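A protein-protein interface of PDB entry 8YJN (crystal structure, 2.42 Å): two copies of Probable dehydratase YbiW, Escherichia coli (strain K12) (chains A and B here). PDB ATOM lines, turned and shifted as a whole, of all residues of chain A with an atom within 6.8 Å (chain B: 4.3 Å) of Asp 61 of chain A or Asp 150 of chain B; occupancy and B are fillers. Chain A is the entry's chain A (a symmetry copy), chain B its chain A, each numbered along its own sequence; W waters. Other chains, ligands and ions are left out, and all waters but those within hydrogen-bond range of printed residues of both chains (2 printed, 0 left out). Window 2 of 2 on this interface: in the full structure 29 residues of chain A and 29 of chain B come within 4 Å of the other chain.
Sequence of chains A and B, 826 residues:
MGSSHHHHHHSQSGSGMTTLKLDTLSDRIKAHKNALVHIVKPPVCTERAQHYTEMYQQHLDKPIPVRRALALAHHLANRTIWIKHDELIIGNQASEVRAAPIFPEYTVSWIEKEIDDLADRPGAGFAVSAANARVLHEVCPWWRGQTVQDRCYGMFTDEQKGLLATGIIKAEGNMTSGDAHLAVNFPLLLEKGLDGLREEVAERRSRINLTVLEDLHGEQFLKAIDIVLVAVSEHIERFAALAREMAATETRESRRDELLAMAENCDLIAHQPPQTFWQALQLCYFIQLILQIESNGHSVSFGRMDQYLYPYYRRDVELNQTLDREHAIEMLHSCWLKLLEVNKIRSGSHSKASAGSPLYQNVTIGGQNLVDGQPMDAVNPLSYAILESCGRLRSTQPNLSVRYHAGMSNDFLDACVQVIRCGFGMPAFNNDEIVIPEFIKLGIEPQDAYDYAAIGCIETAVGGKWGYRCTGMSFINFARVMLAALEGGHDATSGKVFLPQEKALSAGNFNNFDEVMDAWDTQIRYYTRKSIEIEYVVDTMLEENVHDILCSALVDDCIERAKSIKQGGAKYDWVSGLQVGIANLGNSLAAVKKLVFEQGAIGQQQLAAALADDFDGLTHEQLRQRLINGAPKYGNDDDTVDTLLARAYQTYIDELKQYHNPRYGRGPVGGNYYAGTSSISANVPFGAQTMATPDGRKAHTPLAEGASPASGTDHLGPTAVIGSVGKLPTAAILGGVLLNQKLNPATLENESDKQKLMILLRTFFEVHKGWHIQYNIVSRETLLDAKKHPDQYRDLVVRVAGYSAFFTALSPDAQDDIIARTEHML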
ATOM      1  N   TYR A  56      -2.454  10.034  13.403  1.00  0.00           N
ATOM      2  CA  TYR A  56      -3.100   9.061  14.275  1.00  0.00           C
ATOM      3  C   TYR A  56      -2.843   7.651  13.778  1.00  0.00           C
ATOM      4  O   TYR A  56      -2.633   6.729  14.574  1.00  0.00           O
ATOM      5  CB  TYR A  56      -4.601   9.310  14.369  1.00  0.00           C
ATOM      6  CG  TYR A  56      -5.048  10.129  15.563  1.00  0.00           C
ATOM      7  CD1 TYR A  56      -4.588  11.436  15.752  1.00  0.00           C
ATOM      8  CD2 TYR A  56      -5.975   9.625  16.464  1.00  0.00           C
ATOM      9  CE1 TYR A  56      -5.004  12.188  16.816  1.00  0.00           C
ATOM     10  CE2 TYR A  56      -6.411  10.377  17.539  1.00  0.00           C
ATOM     11  CZ  TYR A  56      -5.921  11.663  17.718  1.00  0.00           C
ATOM     12  OH  TYR A  56      -6.353  12.446  18.792  1.00  0.00           O
ATOM     13  N   GLN A  57      -2.845   7.469  12.457  1.00  0.00           N
ATOM     14  CA  GLN A  57      -2.717   6.132  11.896  1.00  0.00           C
ATOM     15  C   GLN A  57      -1.305   5.594  12.060  1.00  0.00           C
ATOM     16  O   GLN A  57      -1.116   4.421  12.387  1.00  0.00           O
ATOM     17  CB  GLN A  57      -3.128   6.152  10.430  1.00  0.00           C
ATOM     18  CG  GLN A  57      -4.599   5.881  10.235  1.00  0.00           C
ATOM     19  CD  GLN A  57      -5.091   6.313   8.884  1.00  0.00           C
ATOM     20  OE1 GLN A  57      -4.366   6.940   8.114  1.00  0.00           O
ATOM     21  NE2 GLN A  57      -6.336   5.989   8.584  1.00  0.00           N
ATOM     22  N   GLN A  58      -0.306   6.440  11.864  1.00  0.00           N
ATOM     23  CA  GLN A  58       1.075   6.009  11.960  1.00  0.00           C
ATOM     24  C   GLN A  58       1.556   5.936  13.402  1.00  0.00           C
ATOM     25  O   GLN A  58       2.543   5.248  13.684  1.00  0.00           O
ATOM     26  CB  GLN A  58       1.939   6.961  11.133  1.00  0.00           C
ATOM     27  CG  GLN A  58       3.378   7.140  11.604  1.00  0.00           C
ATOM     28  CD  GLN A  58       4.193   8.066  10.690  1.00  0.00           C
ATOM     29  OE1 GLN A  58       3.688   8.570   9.670  1.00  0.00           O
ATOM     30  NE2 GLN A  58       5.461   8.293  11.058  1.00  0.00           N
ATOM     31  N   HIS A  59       0.861   6.588  14.329  1.00  0.00           N
ATOM     32  CA  HIS A  59       1.296   6.683  15.714  1.00  0.00           C
ATOM     33  C   HIS A  59       0.245   6.110  16.660  1.00  0.00           C
ATOM     34  O   HIS A  59       0.125   6.531  17.815  1.00  0.00           O
ATOM     35  CB  HIS A  59       1.646   8.129  16.061  1.00  0.00           C
ATOM     36  CG  HIS A  59       2.898   8.619  15.388  1.00  0.00           C
ATOM     37  ND1 HIS A  59       4.141   8.075  15.637  1.00  0.00           N
ATOM     38  CD2 HIS A  59       3.095   9.591  14.462  1.00  0.00           C
ATOM     39  CE1 HIS A  59       5.050   8.702  14.909  1.00  0.00           C
ATOM     40  NE2 HIS A  59       4.441   9.627  14.187  1.00  0.00           N
ATOM     41  N   LEU A  60      -0.520   5.136  16.161  1.00  0.00           N
ATOM     42  CA  LEU A  60      -1.413   4.348  17.002  1.00  0.00           C
ATOM     43  C   LEU A  60      -0.712   3.760  18.225  1.00  0.00           C
ATOM     44  O   LEU A  60      -1.351   3.534  19.262  1.00  0.00           O
ATOM     45  CB  LEU A  60      -2.005   3.224  16.166  1.00  0.00           C
ATOM     46  CG  LEU A  60      -3.485   3.293  15.860  1.00  0.00           C
ATOM     47  CD1 LEU A  60      -3.930   1.901  15.502  1.00  0.00           C
ATOM     48  CD2 LEU A  60      -4.196   3.772  17.088  1.00  0.00           C
ATOM     49  N   ASP A  61       0.594   3.481  18.113  1.00  0.00           N
ATOM     50  CA  ASP A  61       1.380   2.922  19.207  1.00  0.00           C
ATOM     51  C   ASP A  61       1.749   3.955  20.273  1.00  0.00           C
ATOM     52  O   ASP A  61       2.081   3.575  21.399  1.00  0.00           O
ATOM     53  CB  ASP A  61       2.645   2.262  18.639  1.00  0.00           C
ATOM     54  CG  ASP A  61       3.607   3.259  18.001  1.00  0.00           C
ATOM     55  OD1 ASP A  61       3.164   4.291  17.445  1.00  0.00           O
ATOM     56  OD2 ASP A  61       4.833   3.013  18.059  1.00  0.00           O
ATOM     57  N   LYS A  62       1.691   5.239  19.961  1.00  0.00           N
ATOM     58  CA  LYS A  62       2.097   6.241  20.939  1.00  0.00           C
ATOM     59  C   LYS A  62       0.960   6.569  21.911  1.00  0.00           C
ATOM     60  O   LYS A  62      -0.220   6.447  21.566  1.00  0.00           O
ATOM     61  CB  LYS A  62       2.544   7.523  20.238  1.00  0.00           C
ATOM     62  CG  LYS A  62       3.505   7.288  19.091  1.00  0.00           C
ATOM     63  CD  LYS A  62       4.855   6.815  19.584  1.00  0.00           C
ATOM     64  CE  LYS A  62       5.887   6.893  18.472  1.00  0.00           C
ATOM     65  NZ  LYS A  62       5.475   6.098  17.276  1.00  0.00           N
ATOM     66  N   PRO A  63       1.295   6.995  23.130  1.00  0.00           N
ATOM     67  CA  PRO A  63       0.264   7.513  24.031  1.00  0.00           C
ATOM     68  C   PRO A  63      -0.446   8.684  23.388  1.00  0.00           C
ATOM     69  O   PRO A  63       0.155   9.463  22.649  1.00  0.00           O
ATOM     70  CB  PRO A  63       1.059   7.952  25.262  1.00  0.00           C
ATOM     71  CG  PRO A  63       2.267   7.132  25.223  1.00  0.00           C
ATOM     72  CD  PRO A  63       2.621   7.008  23.769  1.00  0.00           C
ATOM     73  N   ARG A  67       0.818  11.069  20.537  1.00  0.00           N
ATOM     74  CA  ARG A  67       0.190  11.023  19.226  1.00  0.00           C
ATOM     75  C   ARG A  67      -0.334  12.404  18.810  1.00  0.00           C
ATOM     76  O   ARG A  67      -0.050  12.885  17.707  1.00  0.00           O
ATOM     77  CB  ARG A  67      -0.937   9.997  19.247  1.00  0.00           C
ATOM     78  CG  ARG A  67      -1.476   9.666  17.891  1.00  0.00           C
ATOM     79  CD  ARG A  67      -2.650   8.721  18.020  1.00  0.00           C
ATOM     80  NE  ARG A  67      -2.364   7.596  18.900  1.00  0.00           N
ATOM     81  CZ  ARG A  67      -3.300   6.935  19.566  1.00  0.00           C
ATOM     82  NH1 ARG A  67      -4.580   7.244  19.434  1.00  0.00           N
ATOM     83  NH2 ARG A  67      -2.945   5.956  20.394  1.00  0.00           N
ATOM     84  N   SER B 109       3.098  -9.448  16.370  1.00  0.00           N
ATOM     85  CA  SER B 109       4.428  -9.322  15.771  1.00  0.00           C
ATOM     86  C   SER B 109       5.009 -10.687  15.392  1.00  0.00           C
ATOM     87  O   SER B 109       5.364 -10.923  14.229  1.00  0.00           O
ATOM     88  CB  SER B 109       5.366  -8.597  16.738  1.00  0.00           C
ATOM     89  OG  SER B 109       4.834  -7.330  17.129  1.00  0.00           O
ATOM     90  N   ARG B 144      -2.046  -3.981  14.263  1.00  0.00           N
ATOM     91  CA  ARG B 144      -0.778  -3.268  14.296  1.00  0.00           C
ATOM     92  C   ARG B 144      -0.954  -1.907  14.944  1.00  0.00           C
ATOM     93  O   ARG B 144      -1.900  -1.178  14.634  1.00  0.00           O
ATOM     94  CB  ARG B 144      -0.232  -3.109  12.882  1.00  0.00           C
ATOM     95  CG  ARG B 144       0.182  -4.402  12.239  1.00  0.00           C
ATOM     96  CD  ARG B 144       0.697  -4.160  10.835  1.00  0.00           C
ATOM     97  NE  ARG B 144       0.759  -5.419  10.108  1.00  0.00           N
ATOM     98  CZ  ARG B 144       0.513  -5.559   8.814  1.00  0.00           C
ATOM     99  NH1 ARG B 144       0.230  -4.515   8.044  1.00  0.00           N
ATOM    100  NH2 ARG B 144       0.553  -6.776   8.278  1.00  0.00           N
ATOM    101  N   GLY B 145      -0.032  -1.560  15.838  1.00  0.00           N
ATOM    102  CA  GLY B 145      -0.120  -0.335  16.591  1.00  0.00           C
ATOM    103  C   GLY B 145      -1.003  -0.400  17.820  1.00  0.00           C
ATOM    104  O   GLY B 145      -0.869   0.452  18.700  1.00  0.00           O
ATOM    105  N   THR B 147      -1.540  -3.400  19.745  1.00  0.00           N
ATOM    106  CA  THR B 147      -1.271  -4.480  20.670  1.00  0.00           C
ATOM    107  C   THR B 147      -0.534  -3.957  21.903  1.00  0.00           C
ATOM    108  O   THR B 147       0.109  -2.904  21.878  1.00  0.00           O
ATOM    109  CB  THR B 147      -0.445  -5.539  19.974  1.00  0.00           C
ATOM    110  OG1 THR B 147       0.792  -4.930  19.564  1.00  0.00           O
ATOM    111  CG2 THR B 147      -1.204  -6.033  18.746  1.00  0.00           C
ATOM    112  N   VAL B 148      -0.628  -4.720  22.993  1.00  0.00           N
ATOM    113  CA  VAL B 148       0.203  -4.443  24.165  1.00  0.00           C
ATOM    114  C   VAL B 148       1.663  -4.270  23.755  1.00  0.00           C
ATOM    115  O   VAL B 148       2.326  -3.308  24.155  1.00  0.00           O
ATOM    116  CB  VAL B 148       0.041  -5.558  25.212  1.00  0.00           C
ATOM    117  CG1 VAL B 148       1.007  -5.355  26.395  1.00  0.00           C
ATOM    118  CG2 VAL B 148      -1.398  -5.622  25.685  1.00  0.00           C
ATOM    119  N   GLN B 149       2.185  -5.179  22.920  1.00  0.00           N
ATOM    120  CA  GLN B 149       3.618  -5.122  22.620  1.00  0.00           C
ATOM    121  C   GLN B 149       3.976  -3.869  21.812  1.00  0.00           C
ATOM    122  O   GLN B 149       4.978  -3.205  22.105  1.00  0.00           O
ATOM    123  CB  GLN B 149       4.073  -6.405  21.906  1.00  0.00           C
ATOM    124  CG  GLN B 149       5.550  -6.404  21.544  1.00  0.00           C
ATOM    125  CD  GLN B 149       6.111  -7.788  21.220  1.00  0.00           C
ATOM    126  OE1 GLN B 149       5.483  -8.601  20.517  1.00  0.00           O
ATOM    127  NE2 GLN B 149       7.311  -8.060  21.729  1.00  0.00           N
ATOM    128  N   ASP B 150       3.169  -3.520  20.804  1.00  0.00           N
ATOM    129  CA  ASP B 150       3.413  -2.290  20.050  1.00  0.00           C
ATOM    130  C   ASP B 150       3.316  -1.062  20.952  1.00  0.00           C
ATOM    131  O   ASP B 150       4.119  -0.122  20.840  1.00  0.00           O
ATOM    132  CB  ASP B 150       2.407  -2.160  18.898  1.00  0.00           C
ATOM    133  CG  ASP B 150       2.780  -2.988  17.700  1.00  0.00           C
ATOM    134  OD1 ASP B 150       3.910  -3.510  17.675  1.00  0.00           O
ATOM    135  OD2 ASP B 150       1.951  -3.117  16.775  1.00  0.00           O
ATOM    136  N   ARG B 151       2.319  -1.039  21.839  1.00  0.00           N
ATOM    137  CA  ARG B 151       2.179   0.116  22.709  1.00  0.00           C
ATOM    138  C   ARG B 151       3.337   0.208  23.699  1.00  0.00           C
ATOM    139  O   ARG B 151       3.751   1.321  24.058  1.00  0.00           O
ATOM    140  CB  ARG B 151       0.826   0.067  23.407  1.00  0.00           C
ATOM    141  CG  ARG B 151      -0.331   0.183  22.405  1.00  0.00           C
ATOM    142  CD  ARG B 151      -1.287   1.257  22.789  1.00  0.00           C
ATOM    143  NE  ARG B 151      -1.952   1.827  21.627  1.00  0.00           N
ATOM    144  CZ  ARG B 151      -3.248   1.698  21.372  1.00  0.00           C
ATOM    145  NH1 ARG B 151      -4.056   1.048  22.198  1.00  0.00           N
ATOM    146  NH2 ARG B 151      -3.737   2.208  20.249  1.00  0.00           N
ATOM    147  N   CYS B 152       3.903  -0.934  24.108  1.00  0.00           N
ATOM    148  CA  CYS B 152       5.148  -0.899  24.882  1.00  0.00           C
ATOM    149  C   CYS B 152       6.254  -0.182  24.120  1.00  0.00           C
ATOM    150  O   CYS B 152       6.885   0.748  24.640  1.00  0.00           O
ATOM    151  CB  CYS B 152       5.599  -2.313  25.249  1.00  0.00           C
ATOM    152  SG  CYS B 152       4.565  -3.060  26.484  1.00  0.00           S
ATOM    153  N   TYR B 153       6.500  -0.596  22.877  1.00  0.00           N
ATOM    154  CA  TYR B 153       7.548   0.051  22.095  1.00  0.00           C
ATOM    155  C   TYR B 153       7.197   1.490  21.731  1.00  0.00           C
ATOM    156  O   TYR B 153       8.098   2.288  21.456  1.00  0.00           O
ATOM    157  CB  TYR B 153       7.878  -0.805  20.854  1.00  0.00           C
ATOM    158  CG  TYR B 153       8.797  -1.936  21.254  1.00  0.00           C
ATOM    159  CD1 TYR B 153       8.285  -3.096  21.810  1.00  0.00           C
ATOM    160  CD2 TYR B 153      10.170  -1.823  21.143  1.00  0.00           C
ATOM    161  CE1 TYR B 153       9.101  -4.121  22.210  1.00  0.00           C
ATOM    162  CE2 TYR B 153      11.015  -2.864  21.552  1.00  0.00           C
ATOM    163  CZ  TYR B 153      10.470  -4.001  22.091  1.00  0.00           C
ATOM    164  OH  TYR B 153      11.276  -5.040  22.510  1.00  0.00           O
ATOM    165  N   GLY B 154       5.917   1.855  21.752  1.00  0.00           N
ATOM    166  CA  GLY B 154       5.605   3.265  21.635  1.00  0.00           C
ATOM    167  C   GLY B 154       5.989   4.091  22.846  1.00  0.00           C
ATOM    168  O   GLY B 154       5.931   5.323  22.778  1.00  0.00           O
HETATM  169  O   HOH W   1       5.475   0.286  18.369  1.00  0.00           O
HETATM  170  O   HOH W   2       2.160   3.691  24.030  1.00  0.00           O
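The guanidinium group (NH2) of Arg 151 of chain B is in hydrogen-bond range of the backbone carbonyl oxygen (O) of Leu 60 of chain A, at 2.9 Å. O of Gly 145 of chain B sits close to N of Asp 61 of chain A, at 3.4 Å. The backbone carbonyl oxygen (O) of Leu 60 of chain A sits close to the backbone carbonyl oxygen (O) of Gly 145 of chain B (3.2 Å).
O of Lys 62 of chain A lies within hydrogen-bond range of NH2 of Arg 67 of chain A, at 3.0 Å. OD1 of Asp 61 of chain A lies within salt-bridge range of NZ of Lys 62 of chain A, at 2.9 Å. The backbone NH (N) of Asp 150 of chain B is in hydrogen-bond range of the side-chain hydroxyl (OG1) of Thr 147 of chain B (3.0 Å). ND1 of His 59 of chain A lies within hydrogen-bond range of NZ of Lys 62 of chain A (2.9 Å). The backbone NH (N) of Gly 145 of chain B is in hydrogen-bond range of the side-chain carboxylate (OD2) of Asp 150 of chain B (2.7 Å). The backbone carbonyl oxygen of Gly 145 of chain B lies within hydrogen-bond range of the guanidinium group of Arg 151 of chain B, 3.4 Å away.
CD1 of Leu 60 of chain A touches O of Arg 144 of chain B, at 3.8 Å. CB of Asp 61 of chain A touches O of Asp 150 of chain B, 3.6 Å away. Arg 151 of chain B touches Asp 61 of chain A (CA to O, 3.7 Å). Asp 61 of chain A touches Gly 154 of chain B. O of Gly 154 of chain B touches CD of Lys 62 of chain A, at 3.7 Å. CD of Pro 63 of chain A touches O of Gly 154 of chain B, at 3.8 Å. NH2 of Arg 67 of chain A touches NH2 of Arg 151 of chain B, at 3.8 Å.
Of chain B, only Gly 145, Asp 150, Arg 151 and Gly 154 come within 4 Å of Asp 61 of chain A. Of the printed residues of chain B, Lys 62 of chain A touches Gly 154. Printed residues of chain B within 4 Å of Pro 63 of chain A: Gly 154 (3.8 Å). Ser 109 of chain B touches none of the printed residues of chain A. Gln 149 of chain B touches none of the printed residues of chain A. The nearest residue of chain A that does not touch Asp 150 of chain B is Lys 62 of chain A (6.0 Å).
Printed residues of chain B that touch a printed residue of chain A: Arg 144, Gly 145, Asp 150, Arg 151 and Gly 154. Among the printed residues, no Asp or Glu carboxylate lies within 4 Å of a Lys or Arg side-chain nitrogen of the other chain.
No position is printed for both chains.
Water W2 bridges O of Asp 61 of chain A and O of Arg 151 of chain B. Water W1 bridges OD2 of Asp 61 of chain A (2.8 Å) and O of Asp 150 of chain B (2.8 Å).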
